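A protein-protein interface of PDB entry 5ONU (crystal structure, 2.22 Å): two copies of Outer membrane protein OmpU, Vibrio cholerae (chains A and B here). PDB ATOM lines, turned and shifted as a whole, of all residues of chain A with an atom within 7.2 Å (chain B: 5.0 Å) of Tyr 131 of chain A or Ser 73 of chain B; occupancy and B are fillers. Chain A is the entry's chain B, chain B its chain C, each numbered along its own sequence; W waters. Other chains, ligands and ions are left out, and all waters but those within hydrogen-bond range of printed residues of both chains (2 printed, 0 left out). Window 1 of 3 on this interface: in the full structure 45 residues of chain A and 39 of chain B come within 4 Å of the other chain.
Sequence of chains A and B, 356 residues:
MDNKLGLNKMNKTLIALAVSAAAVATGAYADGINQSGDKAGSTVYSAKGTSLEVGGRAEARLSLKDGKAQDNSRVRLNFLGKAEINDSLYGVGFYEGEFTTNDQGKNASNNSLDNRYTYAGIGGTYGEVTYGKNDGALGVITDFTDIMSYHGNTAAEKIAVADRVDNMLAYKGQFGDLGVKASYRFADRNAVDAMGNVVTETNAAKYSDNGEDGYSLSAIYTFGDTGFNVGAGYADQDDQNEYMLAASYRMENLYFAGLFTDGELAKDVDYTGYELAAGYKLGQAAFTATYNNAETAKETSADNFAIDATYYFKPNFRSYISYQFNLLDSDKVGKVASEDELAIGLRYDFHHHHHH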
ATOM      1  N   THR A 118     -30.910  13.178  30.087  1.00  0.00           N
ATOM      2  CA  THR A 118     -29.464  12.970  30.228  1.00  0.00           C
ATOM      3  C   THR A 118     -28.735  13.531  29.019  1.00  0.00           C
ATOM      4  O   THR A 118     -28.643  12.864  27.995  1.00  0.00           O
ATOM      5  CB  THR A 118     -29.070  11.469  30.371  1.00  0.00           C
ATOM      6  OG1 THR A 118     -29.586  10.722  29.262  1.00  0.00           O
ATOM      7  CG2 THR A 118     -29.580  10.860  31.674  1.00  0.00           C
ATOM      8  N   TYR A 119     -28.191  14.736  29.139  1.00  0.00           N
ATOM      9  CA  TYR A 119     -27.543  15.351  27.987  1.00  0.00           C
ATOM     10  C   TYR A 119     -26.403  16.295  28.338  1.00  0.00           C
ATOM     11  O   TYR A 119     -26.271  16.746  29.477  1.00  0.00           O
ATOM     12  CB  TYR A 119     -28.582  16.096  27.134  1.00  0.00           C
ATOM     13  CG  TYR A 119     -29.147  17.372  27.736  1.00  0.00           C
ATOM     14  CD1 TYR A 119     -28.429  18.565  27.709  1.00  0.00           C
ATOM     15  CD2 TYR A 119     -30.411  17.386  28.311  1.00  0.00           C
ATOM     16  CE1 TYR A 119     -28.947  19.727  28.250  1.00  0.00           C
ATOM     17  CE2 TYR A 119     -30.938  18.544  28.852  1.00  0.00           C
ATOM     18  CZ  TYR A 119     -30.202  19.711  28.819  1.00  0.00           C
ATOM     19  OH  TYR A 119     -30.725  20.864  29.359  1.00  0.00           O
ATOM     20  N   ALA A 120     -25.581  16.584  27.334  1.00  0.00           N
ATOM     21  CA  ALA A 120     -24.574  17.633  27.440  1.00  0.00           C
ATOM     22  C   ALA A 120     -24.608  18.475  26.171  1.00  0.00           C
ATOM     23  O   ALA A 120     -25.074  18.008  25.131  1.00  0.00           O
ATOM     24  CB  ALA A 120     -23.193  17.041  27.664  1.00  0.00           C
ATOM     25  N   GLY A 121     -24.113  19.708  26.243  1.00  0.00           N
ATOM     26  CA  GLY A 121     -24.198  20.596  25.098  1.00  0.00           C
ATOM     27  C   GLY A 121     -23.335  21.843  25.127  1.00  0.00           C
ATOM     28  O   GLY A 121     -22.608  22.098  26.090  1.00  0.00           O
ATOM     29  N   ILE A 122     -23.424  22.620  24.050  1.00  0.00           N
ATOM     30  CA  ILE A 122     -22.667  23.859  23.898  1.00  0.00           C
ATOM     31  C   ILE A 122     -23.583  24.954  23.351  1.00  0.00           C
ATOM     32  O   ILE A 122     -24.463  24.686  22.527  1.00  0.00           O
ATOM     33  CB  ILE A 122     -21.454  23.692  22.946  1.00  0.00           C
ATOM     34  CG1 ILE A 122     -20.631  22.456  23.311  1.00  0.00           C
ATOM     35  CG2 ILE A 122     -20.573  24.934  22.966  1.00  0.00           C
ATOM     36  CD1 ILE A 122     -19.356  22.316  22.504  1.00  0.00           C
ATOM     37  N   VAL A 129     -26.964  23.778  21.296  1.00  0.00           N
ATOM     38  CA  VAL A 129     -27.028  22.422  20.744  1.00  0.00           C
ATOM     39  C   VAL A 129     -26.625  21.372  21.782  1.00  0.00           C
ATOM     40  O   VAL A 129     -25.629  21.546  22.485  1.00  0.00           O
ATOM     41  CB  VAL A 129     -26.114  22.266  19.509  1.00  0.00           C
ATOM     42  CG1 VAL A 129     -26.380  20.937  18.814  1.00  0.00           C
ATOM     43  CG2 VAL A 129     -26.304  23.425  18.543  1.00  0.00           C
ATOM     44  N   THR A 130     -27.393  20.286  21.874  1.00  0.00           N
ATOM     45  CA  THR A 130     -27.120  19.222  22.843  1.00  0.00           C
ATOM     46  C   THR A 130     -27.220  17.813  22.251  1.00  0.00           C
ATOM     47  O   THR A 130     -27.873  17.597  21.225  1.00  0.00           O
ATOM     48  CB  THR A 130     -28.091  19.281  24.046  1.00  0.00           C
ATOM     49  OG1 THR A 130     -29.410  18.908  23.622  1.00  0.00           O
ATOM     50  CG2 THR A 130     -28.126  20.674  24.667  1.00  0.00           C
ATOM     51  N   TYR A 131     -26.575  16.861  22.926  1.00  0.00           N
ATOM     52  CA  TYR A 131     -26.739  15.439  22.632  1.00  0.00           C
ATOM     53  C   TYR A 131     -27.031  14.673  23.922  1.00  0.00           C
ATOM     54  O   TYR A 131     -26.539  15.031  25.000  1.00  0.00           O
ATOM     55  CB  TYR A 131     -25.497  14.867  21.940  1.00  0.00           C
ATOM     56  CG  TYR A 131     -25.640  13.415  21.517  1.00  0.00           C
ATOM     57  CD1 TYR A 131     -26.278  13.078  20.329  1.00  0.00           C
ATOM     58  CD2 TYR A 131     -25.129  12.386  22.299  1.00  0.00           C
ATOM     59  CE1 TYR A 131     -26.411  11.757  19.935  1.00  0.00           C
ATOM     60  CE2 TYR A 131     -25.257  11.059  21.911  1.00  0.00           C
ATOM     61  CZ  TYR A 131     -25.898  10.753  20.728  1.00  0.00           C
ATOM     62  OH  TYR A 131     -26.029   9.439  20.336  1.00  0.00           O
ATOM     63  N   GLY A 132     -27.823  13.611  23.790  1.00  0.00           N
ATOM     64  CA  GLY A 132     -28.362  12.884  24.925  1.00  0.00           C
ATOM     65  C   GLY A 132     -29.865  13.093  24.989  1.00  0.00           C
ATOM     66  O   GLY A 132     -30.403  13.901  24.232  1.00  0.00           O
ATOM     67  N   LYS A 133     -30.550  12.377  25.879  1.00  0.00           N
ATOM     68  CA  LYS A 133     -32.004  12.508  25.971  1.00  0.00           C
ATOM     69  C   LYS A 133     -32.424  13.896  26.449  1.00  0.00           C
ATOM     70  O   LYS A 133     -32.093  14.317  27.571  1.00  0.00           O
ATOM     71  CB  LYS A 133     -32.605  11.444  26.893  1.00  0.00           C
ATOM     72  CG  LYS A 133     -34.130  11.484  26.907  1.00  0.00           C
ATOM     73  CD  LYS A 133     -34.747  10.192  27.416  1.00  0.00           C
ATOM     74  CE  LYS A 133     -36.261  10.212  27.238  1.00  0.00           C
ATOM     75  NZ  LYS A 133     -36.886   8.889  27.515  1.00  0.00           N
ATOM     76  N   ASN A 134     -33.183  14.564  25.578  1.00  0.00           N
ATOM     77  CA  ASN A 134     -33.638  15.943  25.742  1.00  0.00           C
ATOM     78  C   ASN A 134     -34.871  16.180  24.856  1.00  0.00           C
ATOM     79  O   ASN A 134     -35.270  15.296  24.097  1.00  0.00           O
ATOM     80  CB  ASN A 134     -32.512  16.920  25.388  1.00  0.00           C
ATOM     81  CG  ASN A 134     -32.807  18.345  25.826  1.00  0.00           C
ATOM     82  OD1 ASN A 134     -33.780  18.601  26.534  1.00  0.00           O
ATOM     83  ND2 ASN A 134     -31.966  19.281  25.398  1.00  0.00           N
ATOM     84  N   ASP A 166     -33.600   9.859  23.267  1.00  0.00           N
ATOM     85  CA  ASP A 166     -32.138   9.900  23.226  1.00  0.00           C
ATOM     86  C   ASP A 166     -31.588   9.652  21.821  1.00  0.00           C
ATOM     87  O   ASP A 166     -32.351   9.594  20.858  1.00  0.00           O
ATOM     88  CB  ASP A 166     -31.546   8.894  24.227  1.00  0.00           C
ATOM     89  CG  ASP A 166     -31.923   7.443  23.927  1.00  0.00           C
ATOM     90  OD1 ASP A 166     -32.268   7.109  22.774  1.00  0.00           O
ATOM     91  OD2 ASP A 166     -31.867   6.623  24.867  1.00  0.00           O
ATOM     92  N   ASN A 167     -30.266   9.525  21.717  1.00  0.00           N
ATOM     93  CA  ASN A 167     -29.583   9.395  20.427  1.00  0.00           C
ATOM     94  C   ASN A 167     -29.940  10.535  19.475  1.00  0.00           C
ATOM     95  O   ASN A 167     -30.028  10.339  18.262  1.00  0.00           O
ATOM     96  CB  ASN A 167     -29.912   8.045  19.779  1.00  0.00           C
ATOM     97  CG  ASN A 167     -28.781   7.519  18.912  1.00  0.00           C
ATOM     98  OD1 ASN A 167     -27.790   8.209  18.676  1.00  0.00           O
ATOM     99  ND2 ASN A 167     -28.930   6.290  18.428  1.00  0.00           N
ATOM    100  N   MET A 168     -30.150  11.724  20.033  1.00  0.00           N
ATOM    101  CA  MET A 168     -30.681  12.850  19.273  1.00  0.00           C
ATOM    102  C   MET A 168     -29.898  14.145  19.489  1.00  0.00           C
ATOM    103  O   MET A 168     -29.559  14.499  20.618  1.00  0.00           O
ATOM    104  CB  MET A 168     -32.152  13.080  19.635  1.00  0.00           C
ATOM    105  CG  MET A 168     -32.785  14.288  18.952  1.00  0.00           C
ATOM    106  SD  MET A 168     -34.583  14.329  19.093  1.00  0.00           S
ATOM    107  CE  MET A 168     -34.785  14.693  20.835  1.00  0.00           C
ATOM    108  N   LEU A 169     -29.611  14.839  18.392  1.00  0.00           N
ATOM    109  CA  LEU A 169     -29.089  16.199  18.444  1.00  0.00           C
ATOM    110  C   LEU A 169     -30.243  17.194  18.513  1.00  0.00           C
ATOM    111  O   LEU A 169     -31.181  17.123  17.707  1.00  0.00           O
ATOM    112  CB  LEU A 169     -28.215  16.498  17.224  1.00  0.00           C
ATOM    113  CG  LEU A 169     -26.882  15.761  17.107  1.00  0.00           C
ATOM    114  CD1 LEU A 169     -26.370  15.818  15.677  1.00  0.00           C
ATOM    115  CD2 LEU A 169     -25.866  16.356  18.067  1.00  0.00           C
ATOM    116  N   ALA A 170     -30.171  18.122  19.467  1.00  0.00           N
ATOM    117  CA  ALA A 170     -31.239  19.103  19.653  1.00  0.00           C
ATOM    118  C   ALA A 170     -30.723  20.542  19.633  1.00  0.00           C
ATOM    119  O   ALA A 170     -29.738  20.868  20.291  1.00  0.00           O
ATOM    120  CB  ALA A 170     -31.977  18.831  20.956  1.00  0.00           C
ATOM    121  N   TYR A 184     -32.607  16.310  15.251  1.00  0.00           N
ATOM    122  CA  TYR A 184     -32.375  15.145  14.399  1.00  0.00           C
ATOM    123  C   TYR A 184     -31.990  13.925  15.223  1.00  0.00           C
ATOM    124  O   TYR A 184     -31.130  14.002  16.096  1.00  0.00           O
ATOM    125  CB  TYR A 184     -31.285  15.422  13.358  1.00  0.00           C
ATOM    126  CG  TYR A 184     -30.875  14.185  12.583  1.00  0.00           C
ATOM    127  CD1 TYR A 184     -31.604  13.756  11.481  1.00  0.00           C
ATOM    128  CD2 TYR A 184     -29.758  13.444  12.956  1.00  0.00           C
ATOM    129  CE1 TYR A 184     -31.235  12.623  10.776  1.00  0.00           C
ATOM    130  CE2 TYR A 184     -29.382  12.312  12.259  1.00  0.00           C
ATOM    131  CZ  TYR A 184     -30.123  11.906  11.170  1.00  0.00           C
ATOM    132  OH  TYR A 184     -29.748  10.780  10.473  1.00  0.00           O
ATOM    133  N   PHE A 186     -30.705   9.835  15.203  1.00  0.00           N
ATOM    134  CA  PHE A 186     -30.112   8.691  14.512  1.00  0.00           C
ATOM    135  C   PHE A 186     -30.923   7.423  14.749  1.00  0.00           C
ATOM    136  O   PHE A 186     -31.545   7.264  15.799  1.00  0.00           O
ATOM    137  CB  PHE A 186     -28.675   8.443  14.984  1.00  0.00           C
ATOM    138  CG  PHE A 186     -27.732   9.582  14.727  1.00  0.00           C
ATOM    139  CD1 PHE A 186     -27.116   9.725  13.495  1.00  0.00           C
ATOM    140  CD2 PHE A 186     -27.437  10.492  15.729  1.00  0.00           C
ATOM    141  CE1 PHE A 186     -26.236  10.766  13.262  1.00  0.00           C
ATOM    142  CE2 PHE A 186     -26.559  11.534  15.502  1.00  0.00           C
ATOM    143  CZ  PHE A 186     -25.958  11.672  14.267  1.00  0.00           C
ATOM    144  N   GLU B  59     -22.085  13.265  30.707  1.00  0.00           N
ATOM    145  CA  GLU B  59     -21.197  12.939  29.598  1.00  0.00           C
ATOM    146  C   GLU B  59     -21.948  12.385  28.391  1.00  0.00           C
ATOM    147  O   GLU B  59     -22.456  11.262  28.420  1.00  0.00           O
ATOM    148  CB  GLU B  59     -20.132  11.937  30.053  1.00  0.00           C
ATOM    149  CG  GLU B  59     -18.978  11.771  29.076  1.00  0.00           C
ATOM    150  CD  GLU B  59     -17.880  10.873  29.617  1.00  0.00           C
ATOM    151  OE1 GLU B  59     -18.085  10.257  30.683  1.00  0.00           O
ATOM    152  OE2 GLU B  59     -16.812  10.786  28.974  1.00  0.00           O
ATOM    153  N   ALA B  60     -22.020  13.190  27.336  1.00  0.00           N
ATOM    154  CA  ALA B  60     -22.633  12.771  26.082  1.00  0.00           C
ATOM    155  C   ALA B  60     -21.620  12.029  25.215  1.00  0.00           C
ATOM    156  O   ALA B  60     -20.522  12.528  24.971  1.00  0.00           O
ATOM    157  CB  ALA B  60     -23.195  13.970  25.337  1.00  0.00           C
ATOM    158  N   ARG B  61     -21.991  10.840  24.754  1.00  0.00           N
ATOM    159  CA  ARG B  61     -21.076   9.988  23.999  1.00  0.00           C
ATOM    160  C   ARG B  61     -21.778   9.299  22.831  1.00  0.00           C
ATOM    161  O   ARG B  61     -22.744   8.559  23.019  1.00  0.00           O
ATOM    162  CB  ARG B  61     -20.433   8.935  24.913  1.00  0.00           C
ATOM    163  CG  ARG B  61     -19.717   9.503  26.132  1.00  0.00           C
ATOM    164  CD  ARG B  61     -18.896   8.442  26.848  1.00  0.00           C
ATOM    165  NE  ARG B  61     -19.725   7.333  27.311  1.00  0.00           N
ATOM    166  CZ  ARG B  61     -19.245   6.196  27.805  1.00  0.00           C
ATOM    167  NH1 ARG B  61     -17.936   6.011  27.903  1.00  0.00           N
ATOM    168  NH2 ARG B  61     -20.078   5.242  28.200  1.00  0.00           N
ATOM    169  N   LEU B  62     -21.280   9.552  21.625  1.00  0.00           N
ATOM    170  CA  LEU B  62     -21.804   8.921  20.421  1.00  0.00           C
ATOM    171  C   LEU B  62     -20.830   7.871  19.902  1.00  0.00           C
ATOM    172  O   LEU B  62     -19.644   8.160  19.682  1.00  0.00           O
ATOM    173  CB  LEU B  62     -22.078   9.967  19.337  1.00  0.00           C
ATOM    174  CG  LEU B  62     -22.375   9.432  17.933  1.00  0.00           C
ATOM    175  CD1 LEU B  62     -23.703   8.691  17.901  1.00  0.00           C
ATOM    176  CD2 LEU B  62     -22.362  10.559  16.911  1.00  0.00           C
ATOM    177  N   GLN B  70     -24.862   4.519  18.133  1.00  0.00           N
ATOM    178  CA  GLN B  70     -25.421   4.138  19.422  1.00  0.00           C
ATOM    179  C   GLN B  70     -25.128   5.210  20.471  1.00  0.00           C
ATOM    180  O   GLN B  70     -24.000   5.712  20.571  1.00  0.00           O
ATOM    181  CB  GLN B  70     -24.872   2.785  19.881  1.00  0.00           C
ATOM    182  CG  GLN B  70     -25.315   2.392  21.283  1.00  0.00           C
ATOM    183  CD  GLN B  70     -25.087   0.925  21.584  1.00  0.00           C
ATOM    184  OE1 GLN B  70     -25.697   0.051  20.967  1.00  0.00           O
ATOM    185  NE2 GLN B  70     -24.207   0.645  22.539  1.00  0.00           N
ATOM    186  N   ASP B  71     -26.159   5.558  21.237  1.00  0.00           N
ATOM    187  CA  ASP B  71     -26.053   6.528  22.321  1.00  0.00           C
ATOM    188  C   ASP B  71     -25.500   5.859  23.579  1.00  0.00           C
ATOM    189  O   ASP B  71     -26.169   5.027  24.194  1.00  0.00           O
ATOM    190  CB  ASP B  71     -27.425   7.156  22.603  1.00  0.00           C
ATOM    191  CG  ASP B  71     -27.359   8.319  23.583  1.00  0.00           C
ATOM    192  OD1 ASP B  71     -26.346   8.469  24.296  1.00  0.00           O
ATOM    193  OD2 ASP B  71     -28.340   9.090  23.643  1.00  0.00           O
ATOM    194  N   ASN B  72     -24.278   6.224  23.955  1.00  0.00           N
ATOM    195  CA  ASN B  72     -23.653   5.690  25.160  1.00  0.00           C
ATOM    196  C   ASN B  72     -23.459   6.742  26.252  1.00  0.00           C
ATOM    197  O   ASN B  72     -22.538   6.638  27.063  1.00  0.00           O
ATOM    198  CB  ASN B  72     -22.304   5.056  24.814  1.00  0.00           C
ATOM    199  CG  ASN B  72     -22.449   3.752  24.053  1.00  0.00           C
ATOM    200  OD1 ASN B  72     -23.508   3.125  24.068  1.00  0.00           O
ATOM    201  ND2 ASN B  72     -21.382   3.337  23.382  1.00  0.00           N
ATOM    202  N   SER B  73     -24.325   7.752  26.267  1.00  0.00           N
ATOM    203  CA  SER B  73     -24.238   8.830  27.252  1.00  0.00           C
ATOM    204  C   SER B  73     -24.459   8.327  28.678  1.00  0.00           C
ATOM    205  O   SER B  73     -25.121   7.310  28.890  1.00  0.00           O
ATOM    206  CB  SER B  73     -25.252   9.930  26.928  1.00  0.00           C
ATOM    207  OG  SER B  73     -25.035  10.458  25.630  1.00  0.00           O
ATOM    208  N   ARG B  74     -23.911   9.047  29.653  1.00  0.00           N
ATOM    209  CA  ARG B  74     -24.043   8.645  31.051  1.00  0.00           C
ATOM    210  C   ARG B  74     -23.954   9.828  32.016  1.00  0.00           C
ATOM    211  O   ARG B  74     -23.238  10.802  31.765  1.00  0.00           O
ATOM    212  CB  ARG B  74     -22.973   7.615  31.413  1.00  0.00           C
ATOM    213  CG  ARG B  74     -21.553   8.121  31.229  1.00  0.00           C
ATOM    214  CD  ARG B  74     -20.533   7.013  31.399  1.00  0.00           C
ATOM    215  NE  ARG B  74     -19.171   7.504  31.214  1.00  0.00           N
ATOM    216  CZ  ARG B  74     -18.081   6.760  31.369  1.00  0.00           C
ATOM    217  NH1 ARG B  74     -18.191   5.486  31.716  1.00  0.00           N
ATOM    218  NH2 ARG B  74     -16.881   7.292  31.181  1.00  0.00           N
ATOM    219  N   VAL B  75     -24.694   9.730  33.117  1.00  0.00           N
ATOM    220  CA  VAL B  75     -24.613  10.701  34.204  1.00  0.00           C
ATOM    221  C   VAL B  75     -24.124  10.025  35.485  1.00  0.00           C
ATOM    222  O   VAL B  75     -24.542   8.910  35.801  1.00  0.00           O
ATOM    223  CB  VAL B  75     -25.986  11.376  34.456  1.00  0.00           C
ATOM    224  CG1 VAL B  75     -26.027  12.059  35.819  1.00  0.00           C
ATOM    225  CG2 VAL B  75     -26.302  12.371  33.350  1.00  0.00           C
ATOM    226  N   PHE B  99     -26.324   6.705  35.976  1.00  0.00           N
ATOM    227  CA  PHE B  99     -27.664   6.732  35.389  1.00  0.00           C
ATOM    228  C   PHE B  99     -27.611   6.782  33.857  1.00  0.00           C
ATOM    229  O   PHE B  99     -26.871   7.585  33.287  1.00  0.00           O
ATOM    230  CB  PHE B  99     -28.453   7.941  35.915  1.00  0.00           C
ATOM    231  CG  PHE B  99     -28.475   8.055  37.420  1.00  0.00           C
ATOM    232  CD1 PHE B  99     -27.388   8.568  38.112  1.00  0.00           C
ATOM    233  CD2 PHE B  99     -29.592   7.663  38.138  1.00  0.00           C
ATOM    234  CE1 PHE B  99     -27.410   8.675  39.492  1.00  0.00           C
ATOM    235  CE2 PHE B  99     -29.621   7.768  39.517  1.00  0.00           C
ATOM    236  CZ  PHE B  99     -28.529   8.275  40.194  1.00  0.00           C
ATOM    237  N   THR B 100     -28.392   5.929  33.195  1.00  0.00           N
ATOM    238  CA  THR B 100     -28.397   5.863  31.729  1.00  0.00           C
ATOM    239  C   THR B 100     -29.802   5.723  31.133  1.00  0.00           C
ATOM    240  O   THR B 100     -30.761   5.424  31.844  1.00  0.00           O
ATOM    241  CB  THR B 100     -27.546   4.682  31.208  1.00  0.00           C
ATOM    242  OG1 THR B 100     -28.064   3.451  31.727  1.00  0.00           O
ATOM    243  CG2 THR B 100     -26.086   4.831  31.618  1.00  0.00           C
HETATM  244  O   HOH W   1     -28.797   3.739  20.761  1.00  0.00           O
HETATM  245  O   HOH W   2     -29.053   9.780  26.616  1.00  0.00           O
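O of Val 75 of chain B is in hydrogen-bond range of N of Phe 99 of chain B, 2.8 Å away. The backbone NH (N) of Lys 133 of chain A sits at hydrogen-bond distance from the backbone carbonyl oxygen (O) of Thr 118 of chain A (2.9 Å). N of Tyr 131 of chain A lies within hydrogen-bond range of O of Ala 120 of chain A (2.9 Å). The guanidinium group (NE) of Arg 61 of chain B lies within hydrogen-bond range of the backbone carbonyl oxygen (O) of Asn 72 of chain B. The backbone NH (N) of Phe 186 of chain A is in hydrogen-bond range of the backbone carbonyl oxygen (O) of Asn 167 of chain A. The side-chain amide oxygen (OD1) of Asn 167 of chain A is in hydrogen-bond range of the side-chain hydroxyl (OH) of Tyr 131 of chain A, 2.7 Å away.
Ser 73 of chain B touches one residue of chain A. Of the printed residues of chain B, Ala 120 of chain A touches Ala 60 (3.9 Å). Printed residues of chain B within 4 Å of Asp 166 of chain A: Asp 71 (3.3 Å). Gln 70 of chain B touches none of the printed residues of chain A. The nearest residue of chain A that does not touch Ser 73 of chain B is Gly 132 of chain A (4.2 Å).
No position is printed for both chains. Of the 9 pairs that touch across the chains among the printed residues, none has its exchanged pair printed and touching as well.
Of the 12 printed residues of chain B, 6 touch a printed residue of chain A. Printed residues of chain B that touch a printed residue of chain A: Ala 60, Arg 61, Leu 62, Asp 71, Ser 73 and Val 75. Hydrophobic or aromatic side chains of chain B within 4 Å of the printed part of chain A: Ala 60, Leu 62 and Val 75. Among the printed residues, 9 pairs touch across the chains. Among the printed residues, no Asp or Glu carboxylate lies within 4 Å of a Lys or Arg side-chain nitrogen of the other chain.
The backbone NH (N) of Asn 167 of chain A sits at hydrogen-bond distance from the side-chain carboxylate (OD2) of Asp 71 of chain B (2.8 Å).
Water W2 lies within hydrogen-bond range of the side-chain hydroxyl (OG1) of Thr 118 of chain A (2.9 Å), the backbone NH (N) of Lys 133 of chain A (3.1 Å) and the side-chain carboxylate (OD2) of Asp 71 of chain B (3.1 Å). Water W1 lies within hydrogen-bond range of the backbone NH (N) of Asp 71 of chain B (3.2 Å) and the side-chain amide nitrogen (ND2) of Asn 167 of chain A (3.5 Å).
Among the printed residues, merely in contact across the chains: Asp 166 of chain A with Asp 71 of chain B (3.3 Å), Tyr 131 of chain A with Leu 62 of chain B (3.4 Å), Tyr 131 of chain A with Asp 71 of chain B (3.5 Å), Tyr 131 of chain A with Ala 60 of chain B (3.5 Å), Tyr 131 of chain A with Arg 61 of chain B (3.7 Å), Tyr 131 of chain A with Ser 73 of chain B (3.8 Å), Ala 120 of chain A with Ala 60 of chain B (3.9 Å) and Thr 118 of chain A with Val 75 of chain B (3.98 Å).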
